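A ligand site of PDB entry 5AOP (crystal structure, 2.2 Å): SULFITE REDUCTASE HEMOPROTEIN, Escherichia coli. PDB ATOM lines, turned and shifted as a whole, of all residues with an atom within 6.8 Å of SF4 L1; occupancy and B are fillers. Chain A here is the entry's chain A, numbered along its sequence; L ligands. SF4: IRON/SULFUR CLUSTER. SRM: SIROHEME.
FE1 of SF4 L1 is bound by SG of Cys 361, at 2.2 Å. N of Cys 410 lies close to S2 of SF4 L1 (3.3 Å). The side-chain sulfur (SG) of Cys 410 is bound to an iron atom (FE4) of SF4 L1 (2.3 Å). An iron atom (FE3) of SF4 L1 is bound by the side-chain sulfur (SG) of Cys 406. SG of Cys 367 binds FE2 of SF4 L1. A sulfur (S2) of SF4 L1 lies close to the side-chain hydroxyl (OG1) of Thr 404 (3.2 Å). The side-chain amide nitrogen of Asn 408 sits close to a sulfur (S1) of SF4 L1 (3.3 Å). N of Ser 363 sits close to S3 of SF4 L1. The backbone NH (N) of Gly 409 sits close to a sulfur (S2) of SF4 L1. FE of SRM L2 is bound by SG of Cys 410 (2.4 Å). The backbone NH (N) of Cys 367 is in hydrogen-bond range of an oxygen (O1A) of SRM L2 (3.3 Å). The backbone NH (N) of Val 362 is in hydrogen-bond range of an oxygen (O3B) of SRM L2, 3.2 Å away.
The side-chain sulfur (SG) of Cys 361 sits close to the backbone NH (N) of Ser 363 (3.8 Å). The backbone NH (N) of Gly 405 lies close to the side-chain sulfur (SG) of Cys 361 (3.1 Å). O of Val 403 is in hydrogen-bond range of N of Cys 361 (3.2 Å). The side-chain sulfur of Cys 406 lies close to the backbone carbonyl oxygen of Leu 369 (3.7 Å). The side-chain sulfur (SG) of Cys 367 lies close to the backbone NH (N) of Leu 369, at 3.5 Å. The side-chain hydroxyl (OG1) of Thr 404 lies within hydrogen-bond range of the backbone NH (N) of Gly 411 (3.0 Å). OG of Ser 363 sits at hydrogen-bond distance from O of Ala 372 (2.7 Å). N of Ala 372 is in hydrogen-bond range of O of Gly 405.
Val 362 touches SF4 L1. Ala 370 touches SF4 L1 (CA to S4, 3.4 Å). Gly 405 touches SF4 L1. Hydrophobic or aromatic side chains within 4 Å of SF4 L1: Ala 370. The nearest printed residue that does not touch SF4 L1 is Leu 369 (4.001 Å).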
ATOM      1  N   ALA A 360       6.740 -16.414   6.751  1.00  0.00           N
ATOM      2  CA  ALA A 360       7.007 -16.890   5.403  1.00  0.00           C
ATOM      3  C   ALA A 360       6.701 -18.395   5.338  1.00  0.00           C
ATOM      4  O   ALA A 360       6.694 -19.085   6.372  1.00  0.00           O
ATOM      5  CB  ALA A 360       8.467 -16.602   5.024  1.00  0.00           C
ATOM      6  N   CYS A 361       6.377 -18.885   4.145  1.00  0.00           N
ATOM      7  CA  CYS A 361       6.110 -20.303   3.935  1.00  0.00           C
ATOM      8  C   CYS A 361       7.456 -21.008   3.707  1.00  0.00           C
ATOM      9  O   CYS A 361       8.498 -20.345   3.575  1.00  0.00           O
ATOM     10  CB  CYS A 361       5.224 -20.513   2.702  1.00  0.00           C
ATOM     11  SG  CYS A 361       6.091 -20.193   1.134  1.00  0.00           S
ATOM     12  N   VAL A 362       7.432 -22.336   3.578  1.00  0.00           N
ATOM     13  CA  VAL A 362       8.641 -23.127   3.336  1.00  0.00           C
ATOM     14  C   VAL A 362       9.357 -22.762   2.018  1.00  0.00           C
ATOM     15  O   VAL A 362      10.545 -22.378   2.015  1.00  0.00           O
ATOM     16  CB  VAL A 362       8.315 -24.612   3.347  1.00  0.00           C
ATOM     17  CG1 VAL A 362       9.534 -25.405   2.991  1.00  0.00           C
ATOM     18  CG2 VAL A 362       7.793 -25.017   4.723  1.00  0.00           C
ATOM     19  N   SER A 363       8.630 -22.947   0.904  1.00  0.00           N
ATOM     20  CA  SER A 363       9.146 -22.657  -0.430  1.00  0.00           C
ATOM     21  C   SER A 363      10.393 -23.524  -0.730  1.00  0.00           C
ATOM     22  O   SER A 363      10.448 -24.691  -0.328  1.00  0.00           O
ATOM     23  CB  SER A 363       9.479 -21.161  -0.548  1.00  0.00           C
ATOM     24  OG  SER A 363       9.761 -20.801  -1.891  1.00  0.00           O
ATOM     25  N   PHE A 364      11.376 -22.947  -1.433  1.00  0.00           N
ATOM     26  CA  PHE A 364      12.601 -23.672  -1.744  1.00  0.00           C
ATOM     27  C   PHE A 364      13.305 -23.954  -0.417  1.00  0.00           C
ATOM     28  O   PHE A 364      13.272 -23.117   0.483  1.00  0.00           O
ATOM     29  CB  PHE A 364      13.539 -22.800  -2.600  1.00  0.00           C
ATOM     30  CG  PHE A 364      13.006 -22.493  -3.953  1.00  0.00           C
ATOM     31  CD1 PHE A 364      12.785 -23.506  -4.869  1.00  0.00           C
ATOM     32  CD2 PHE A 364      12.739 -21.166  -4.323  1.00  0.00           C
ATOM     33  CE1 PHE A 364      12.299 -23.212  -6.149  1.00  0.00           C
ATOM     34  CE2 PHE A 364      12.252 -20.863  -5.607  1.00  0.00           C
ATOM     35  CZ  PHE A 364      12.032 -21.886  -6.520  1.00  0.00           C
ATOM     36  N   CYS A 367       9.875 -27.263  -1.499  1.00  0.00           N
ATOM     37  CA  CYS A 367       8.580 -27.200  -2.162  1.00  0.00           C
ATOM     38  C   CYS A 367       8.688 -27.242  -3.676  1.00  0.00           C
ATOM     39  O   CYS A 367       9.374 -26.448  -4.291  1.00  0.00           O
ATOM     40  CB  CYS A 367       7.812 -25.982  -1.719  1.00  0.00           C
ATOM     41  SG  CYS A 367       6.142 -25.984  -2.393  1.00  0.00           S
ATOM     42  N   PRO A 368       7.972 -28.177  -4.313  1.00  0.00           N
ATOM     43  CA  PRO A 368       7.990 -28.319  -5.769  1.00  0.00           C
ATOM     44  C   PRO A 368       7.203 -27.263  -6.552  1.00  0.00           C
ATOM     45  O   PRO A 368       7.303 -27.158  -7.784  1.00  0.00           O
ATOM     46  CB  PRO A 368       7.393 -29.716  -5.966  1.00  0.00           C
ATOM     47  CG  PRO A 368       6.404 -29.819  -4.812  1.00  0.00           C
ATOM     48  CD  PRO A 368       7.210 -29.267  -3.666  1.00  0.00           C
ATOM     49  N   LEU A 369       6.420 -26.470  -5.834  1.00  0.00           N
ATOM     50  CA  LEU A 369       5.575 -25.464  -6.442  1.00  0.00           C
ATOM     51  C   LEU A 369       6.101 -24.073  -6.232  1.00  0.00           C
ATOM     52  O   LEU A 369       5.529 -23.114  -6.737  1.00  0.00           O
ATOM     53  CB  LEU A 369       4.167 -25.572  -5.845  1.00  0.00           C
ATOM     54  CG  LEU A 369       3.631 -27.006  -5.740  1.00  0.00           C
ATOM     55  CD1 LEU A 369       2.255 -27.021  -5.092  1.00  0.00           C
ATOM     56  CD2 LEU A 369       3.602 -27.626  -7.151  1.00  0.00           C
ATOM     57  N   ALA A 370       7.218 -23.953  -5.508  1.00  0.00           N
ATOM     58  CA  ALA A 370       7.800 -22.649  -5.192  1.00  0.00           C
ATOM     59  C   ALA A 370       8.221 -21.843  -6.413  1.00  0.00           C
ATOM     60  O   ALA A 370       8.866 -22.375  -7.318  1.00  0.00           O
ATOM     61  CB  ALA A 370       8.980 -22.829  -4.271  1.00  0.00           C
ATOM     62  N   MET A 371       7.860 -20.562  -6.437  1.00  0.00           N
ATOM     63  CA  MET A 371       8.215 -19.671  -7.523  1.00  0.00           C
ATOM     64  C   MET A 371       9.345 -18.739  -7.081  1.00  0.00           C
ATOM     65  O   MET A 371      10.264 -18.475  -7.850  1.00  0.00           O
ATOM     66  CB  MET A 371       7.017 -18.876  -8.003  1.00  0.00           C
ATOM     67  CG  MET A 371       5.889 -19.726  -8.626  1.00  0.00           C
ATOM     68  SD  MET A 371       4.434 -18.733  -9.102  1.00  0.00           S
ATOM     69  CE  MET A 371       3.420 -19.903  -9.964  1.00  0.00           C
ATOM     70  N   ALA A 372       9.306 -18.302  -5.826  1.00  0.00           N
ATOM     71  CA  ALA A 372      10.333 -17.408  -5.293  1.00  0.00           C
ATOM     72  C   ALA A 372      10.638 -17.852  -3.868  1.00  0.00           C
ATOM     73  O   ALA A 372       9.819 -18.511  -3.267  1.00  0.00           O
ATOM     74  CB  ALA A 372       9.834 -15.981  -5.293  1.00  0.00           C
ATOM     75  N   ALA A 374      11.117 -17.886   0.157  1.00  0.00           N
ATOM     76  CA  ALA A 374      10.266 -17.358   1.214  1.00  0.00           C
ATOM     77  C   ALA A 374      10.972 -17.530   2.552  1.00  0.00           C
ATOM     78  O   ALA A 374      11.540 -16.572   3.090  1.00  0.00           O
ATOM     79  CB  ALA A 374       8.927 -18.060   1.213  1.00  0.00           C
ATOM     80  N   VAL A 403       5.493 -13.355   3.600  1.00  0.00           N
ATOM     81  CA  VAL A 403       6.002 -13.719   2.303  1.00  0.00           C
ATOM     82  C   VAL A 403       5.601 -15.140   2.003  1.00  0.00           C
ATOM     83  O   VAL A 403       5.803 -16.051   2.802  1.00  0.00           O
ATOM     84  CB  VAL A 403       7.531 -13.614   2.300  1.00  0.00           C
ATOM     85  CG1 VAL A 403       8.089 -13.993   0.931  1.00  0.00           C
ATOM     86  CG2 VAL A 403       7.974 -12.182   2.687  1.00  0.00           C
ATOM     87  N   THR A 404       4.969 -15.330   0.862  1.00  0.00           N
ATOM     88  CA  THR A 404       4.533 -16.651   0.424  1.00  0.00           C
ATOM     89  C   THR A 404       5.259 -16.893  -0.920  1.00  0.00           C
ATOM     90  O   THR A 404       5.373 -15.977  -1.741  1.00  0.00           O
ATOM     91  CB  THR A 404       2.964 -16.715   0.337  1.00  0.00           C
ATOM     92  OG1 THR A 404       2.518 -18.068   0.420  1.00  0.00           O
ATOM     93  CG2 THR A 404       2.430 -16.076  -0.933  1.00  0.00           C
ATOM     94  N   GLY A 405       5.853 -18.069  -1.072  1.00  0.00           N
ATOM     95  CA  GLY A 405       6.610 -18.384  -2.286  1.00  0.00           C
ATOM     96  C   GLY A 405       5.911 -18.557  -3.620  1.00  0.00           C
ATOM     97  O   GLY A 405       6.568 -18.663  -4.655  1.00  0.00           O
ATOM     98  N   CYS A 406       4.584 -18.600  -3.607  1.00  0.00           N
ATOM     99  CA  CYS A 406       3.813 -18.762  -4.838  1.00  0.00           C
ATOM    100  C   CYS A 406       2.379 -18.411  -4.448  1.00  0.00           C
ATOM    101  O   CYS A 406       2.073 -18.289  -3.277  1.00  0.00           O
ATOM    102  CB  CYS A 406       3.947 -20.208  -5.395  1.00  0.00           C
ATOM    103  SG  CYS A 406       2.907 -21.504  -4.674  1.00  0.00           S
ATOM    104  N   PRO A 407       1.473 -18.263  -5.429  1.00  0.00           N
ATOM    105  CA  PRO A 407       0.087 -17.911  -5.128  1.00  0.00           C
ATOM    106  C   PRO A 407      -0.774 -18.872  -4.289  1.00  0.00           C
ATOM    107  O   PRO A 407      -1.870 -18.494  -3.862  1.00  0.00           O
ATOM    108  CB  PRO A 407      -0.492 -17.617  -6.504  1.00  0.00           C
ATOM    109  CG  PRO A 407       0.239 -18.576  -7.361  1.00  0.00           C
ATOM    110  CD  PRO A 407       1.658 -18.433  -6.876  1.00  0.00           C
ATOM    111  N   ASN A 408      -0.309 -20.101  -4.035  1.00  0.00           N
ATOM    112  CA  ASN A 408      -1.061 -21.038  -3.199  1.00  0.00           C
ATOM    113  C   ASN A 408      -1.279 -20.381  -1.832  1.00  0.00           C
ATOM    114  O   ASN A 408      -2.257 -20.674  -1.136  1.00  0.00           O
ATOM    115  CB  ASN A 408      -0.337 -22.375  -3.037  1.00  0.00           C
ATOM    116  CG  ASN A 408      -0.423 -23.228  -4.285  1.00  0.00           C
ATOM    117  OD1 ASN A 408      -1.367 -23.077  -5.062  1.00  0.00           O
ATOM    118  ND2 ASN A 408       0.543 -24.112  -4.481  1.00  0.00           N
ATOM    119  N   GLY A 409      -0.335 -19.516  -1.459  1.00  0.00           N
ATOM    120  CA  GLY A 409      -0.439 -18.726  -0.229  1.00  0.00           C
ATOM    121  C   GLY A 409      -0.253 -19.302   1.164  1.00  0.00           C
ATOM    122  O   GLY A 409      -0.783 -18.749   2.120  1.00  0.00           O
ATOM    123  N   CYS A 410       0.576 -20.328   1.294  1.00  0.00           N
ATOM    124  CA  CYS A 410       0.821 -20.955   2.594  1.00  0.00           C
ATOM    125  C   CYS A 410       1.353 -20.006   3.675  1.00  0.00           C
ATOM    126  O   CYS A 410       1.060 -20.152   4.862  1.00  0.00           O
ATOM    127  CB  CYS A 410       1.755 -22.146   2.408  1.00  0.00           C
ATOM    128  SG  CYS A 410       1.198 -23.235   1.049  1.00  0.00           S
ATOM    129  N   GLY A 411       2.075 -18.972   3.248  1.00  0.00           N
ATOM    130  CA  GLY A 411       2.626 -18.000   4.188  1.00  0.00           C
ATOM    131  C   GLY A 411       1.586 -16.985   4.641  1.00  0.00           C
ATOM    132  O   GLY A 411       1.909 -16.084   5.414  1.00  0.00           O
HETATM  133 FE1  SF4 L   1       5.138 -21.605  -0.311  1.00  0.00          FE
HETATM  134 FE2  SF4 L   1       5.226 -24.050  -1.607  1.00  0.00          FE
HETATM  135 FE3  SF4 L   1       3.806 -22.030  -2.675  1.00  0.00          FE
HETATM  136 FE4  SF4 L   1       2.996 -23.121  -0.304  1.00  0.00          FE
HETATM  137  S1  SF4 L   1       3.041 -24.136  -2.284  1.00  0.00           S
HETATM  138  S2  SF4 L   1       3.036 -20.884  -0.902  1.00  0.00           S
HETATM  139  S3  SF4 L   1       5.046 -23.607   0.674  1.00  0.00           S
HETATM  140  S4  SF4 L   1       6.064 -22.086  -2.325  1.00  0.00           S
HETATM  141 FE   SRM L   2       0.314 -25.193   2.053  1.00  0.00          FE
HETATM  142  CHA SRM L   2       0.612 -27.007  -0.736  1.00  0.00           C
HETATM  143  CHB SRM L   2       3.446 -26.061   3.012  1.00  0.00           C
HETATM  144  CHC SRM L   2      -0.366 -23.974   5.106  1.00  0.00           C
HETATM  145  CHD SRM L   2      -2.458 -23.566   0.790  1.00  0.00           C
HETATM  146  NA  SRM L   2       1.769 -26.406   1.313  1.00  0.00           N
HETATM  147  C1A SRM L   2       1.651 -27.120   0.158  1.00  0.00           C
HETATM  148  C2A SRM L   2       2.819 -28.037   0.040  1.00  0.00           C
HETATM  149  CMA SRM L   2       2.413 -29.291   0.887  1.00  0.00           C
HETATM  150  CDA SRM L   2       3.258 -28.253  -1.433  1.00  0.00           C
HETATM  151  CEA SRM L   2       2.741 -29.458  -2.218  1.00  0.00           C
HETATM  152  O3A SRM L   2       1.517 -29.553  -2.460  1.00  0.00           O
HETATM  153  O4A SRM L   2       3.556 -30.307  -2.612  1.00  0.00           O
HETATM  154  C3A SRM L   2       3.855 -27.248   0.783  1.00  0.00           C
HETATM  155  CAA SRM L   2       4.928 -28.087   1.385  1.00  0.00           C
HETATM  156  CBA SRM L   2       6.257 -27.376   1.246  1.00  0.00           C
HETATM  157  CCA SRM L   2       7.385 -28.106   1.940  1.00  0.00           C
HETATM  158  O1A SRM L   2       8.406 -28.397   1.278  1.00  0.00           O
HETATM  159  O2A SRM L   2       7.275 -28.389   3.147  1.00  0.00           O
HETATM  160  C4A SRM L   2       3.019 -26.539   1.801  1.00  0.00           C
HETATM  161  NB  SRM L   2       1.354 -25.135   3.789  1.00  0.00           N
HETATM  162  C1B SRM L   2       2.692 -25.371   3.931  1.00  0.00           C
HETATM  163  C2B SRM L   2       3.140 -25.134   5.349  1.00  0.00           C
HETATM  164  CMB SRM L   2       4.132 -26.143   5.915  1.00  0.00           C
HETATM  165  CDB SRM L   2       3.768 -23.687   5.211  1.00  0.00           C
HETATM  166  CEB SRM L   2       4.500 -23.057   6.367  1.00  0.00           C
HETATM  167  O3B SRM L   2       5.567 -22.496   6.130  1.00  0.00           O
HETATM  168  O4B SRM L   2       4.025 -23.126   7.507  1.00  0.00           O
HETATM  169  C3B SRM L   2       1.795 -24.805   6.040  1.00  0.00           C
HETATM  170  CAB SRM L   2       1.482 -26.329   6.441  1.00  0.00           C
HETATM  171  CBB SRM L   2       0.122 -26.488   7.058  1.00  0.00           C
HETATM  172  CCB SRM L   2      -0.137 -27.894   7.548  1.00  0.00           C
HETATM  173  O1B SRM L   2       0.428 -28.235   8.601  1.00  0.00           O
HETATM  174  O2B SRM L   2      -0.894 -28.636   6.903  1.00  0.00           O
HETATM  175  C4B SRM L   2       0.772 -24.748   4.954  1.00  0.00           C
HETATM  176  NC  SRM L   2      -1.099 -23.921   2.792  1.00  0.00           N
HETATM  177  C1C SRM L   2      -1.219 -23.567   4.090  1.00  0.00           C
HETATM  178  C2C SRM L   2      -2.023 -22.356   4.142  1.00  0.00           C
HETATM  179  CDC SRM L   2      -2.235 -21.455   5.335  1.00  0.00           C
HETATM  180  CEC SRM L   2      -3.084 -22.072   6.435  1.00  0.00           C
HETATM  181  O3C SRM L   2      -3.704 -23.139   6.224  1.00  0.00           O
HETATM  182  O4C SRM L   2      -3.122 -21.493   7.533  1.00  0.00           O
HETATM  183  C3C SRM L   2      -2.575 -22.176   2.895  1.00  0.00           C
HETATM  184  CAC SRM L   2      -3.482 -21.030   2.501  1.00  0.00           C
HETATM  185  CBC SRM L   2      -4.947 -21.141   2.944  1.00  0.00           C
HETATM  186  CCC SRM L   2      -5.800 -21.931   1.975  1.00  0.00           C
HETATM  187  O1C SRM L   2      -5.777 -23.161   2.044  1.00  0.00           O
HETATM  188  O2C SRM L   2      -6.501 -21.318   1.152  1.00  0.00           O
HETATM  189  C4C SRM L   2      -2.084 -23.241   2.079  1.00  0.00           C
HETATM  190  ND  SRM L   2      -0.806 -25.349   0.375  1.00  0.00           N
HETATM  191  C1D SRM L   2      -1.886 -24.586   0.014  1.00  0.00           C
HETATM  192  C2D SRM L   2      -2.225 -24.954  -1.363  1.00  0.00           C
HETATM  193  CAD SRM L   2      -3.334 -24.376  -2.221  1.00  0.00           C
HETATM  194  CBD SRM L   2      -4.651 -24.879  -1.678  1.00  0.00           C
HETATM  195  CCD SRM L   2      -5.804 -24.570  -2.570  1.00  0.00           C
HETATM  196  O1D SRM L   2      -6.948 -24.558  -2.076  1.00  0.00           O
HETATM  197  O2D SRM L   2      -5.607 -24.328  -3.775  1.00  0.00           O
HETATM  198  C3D SRM L   2      -1.357 -25.956  -1.728  1.00  0.00           C
HETATM  199  CDD SRM L   2      -1.256 -26.676  -3.040  1.00  0.00           C
HETATM  200  CED SRM L   2      -2.275 -27.766  -3.181  1.00  0.00           C
HETATM  201  O3D SRM L   2      -2.630 -28.420  -2.184  1.00  0.00           O
HETATM  202  O4D SRM L   2      -2.723 -27.961  -4.318  1.00  0.00           O
HETATM  203  C4D SRM L   2      -0.504 -26.194  -0.676  1.00  0.00           C
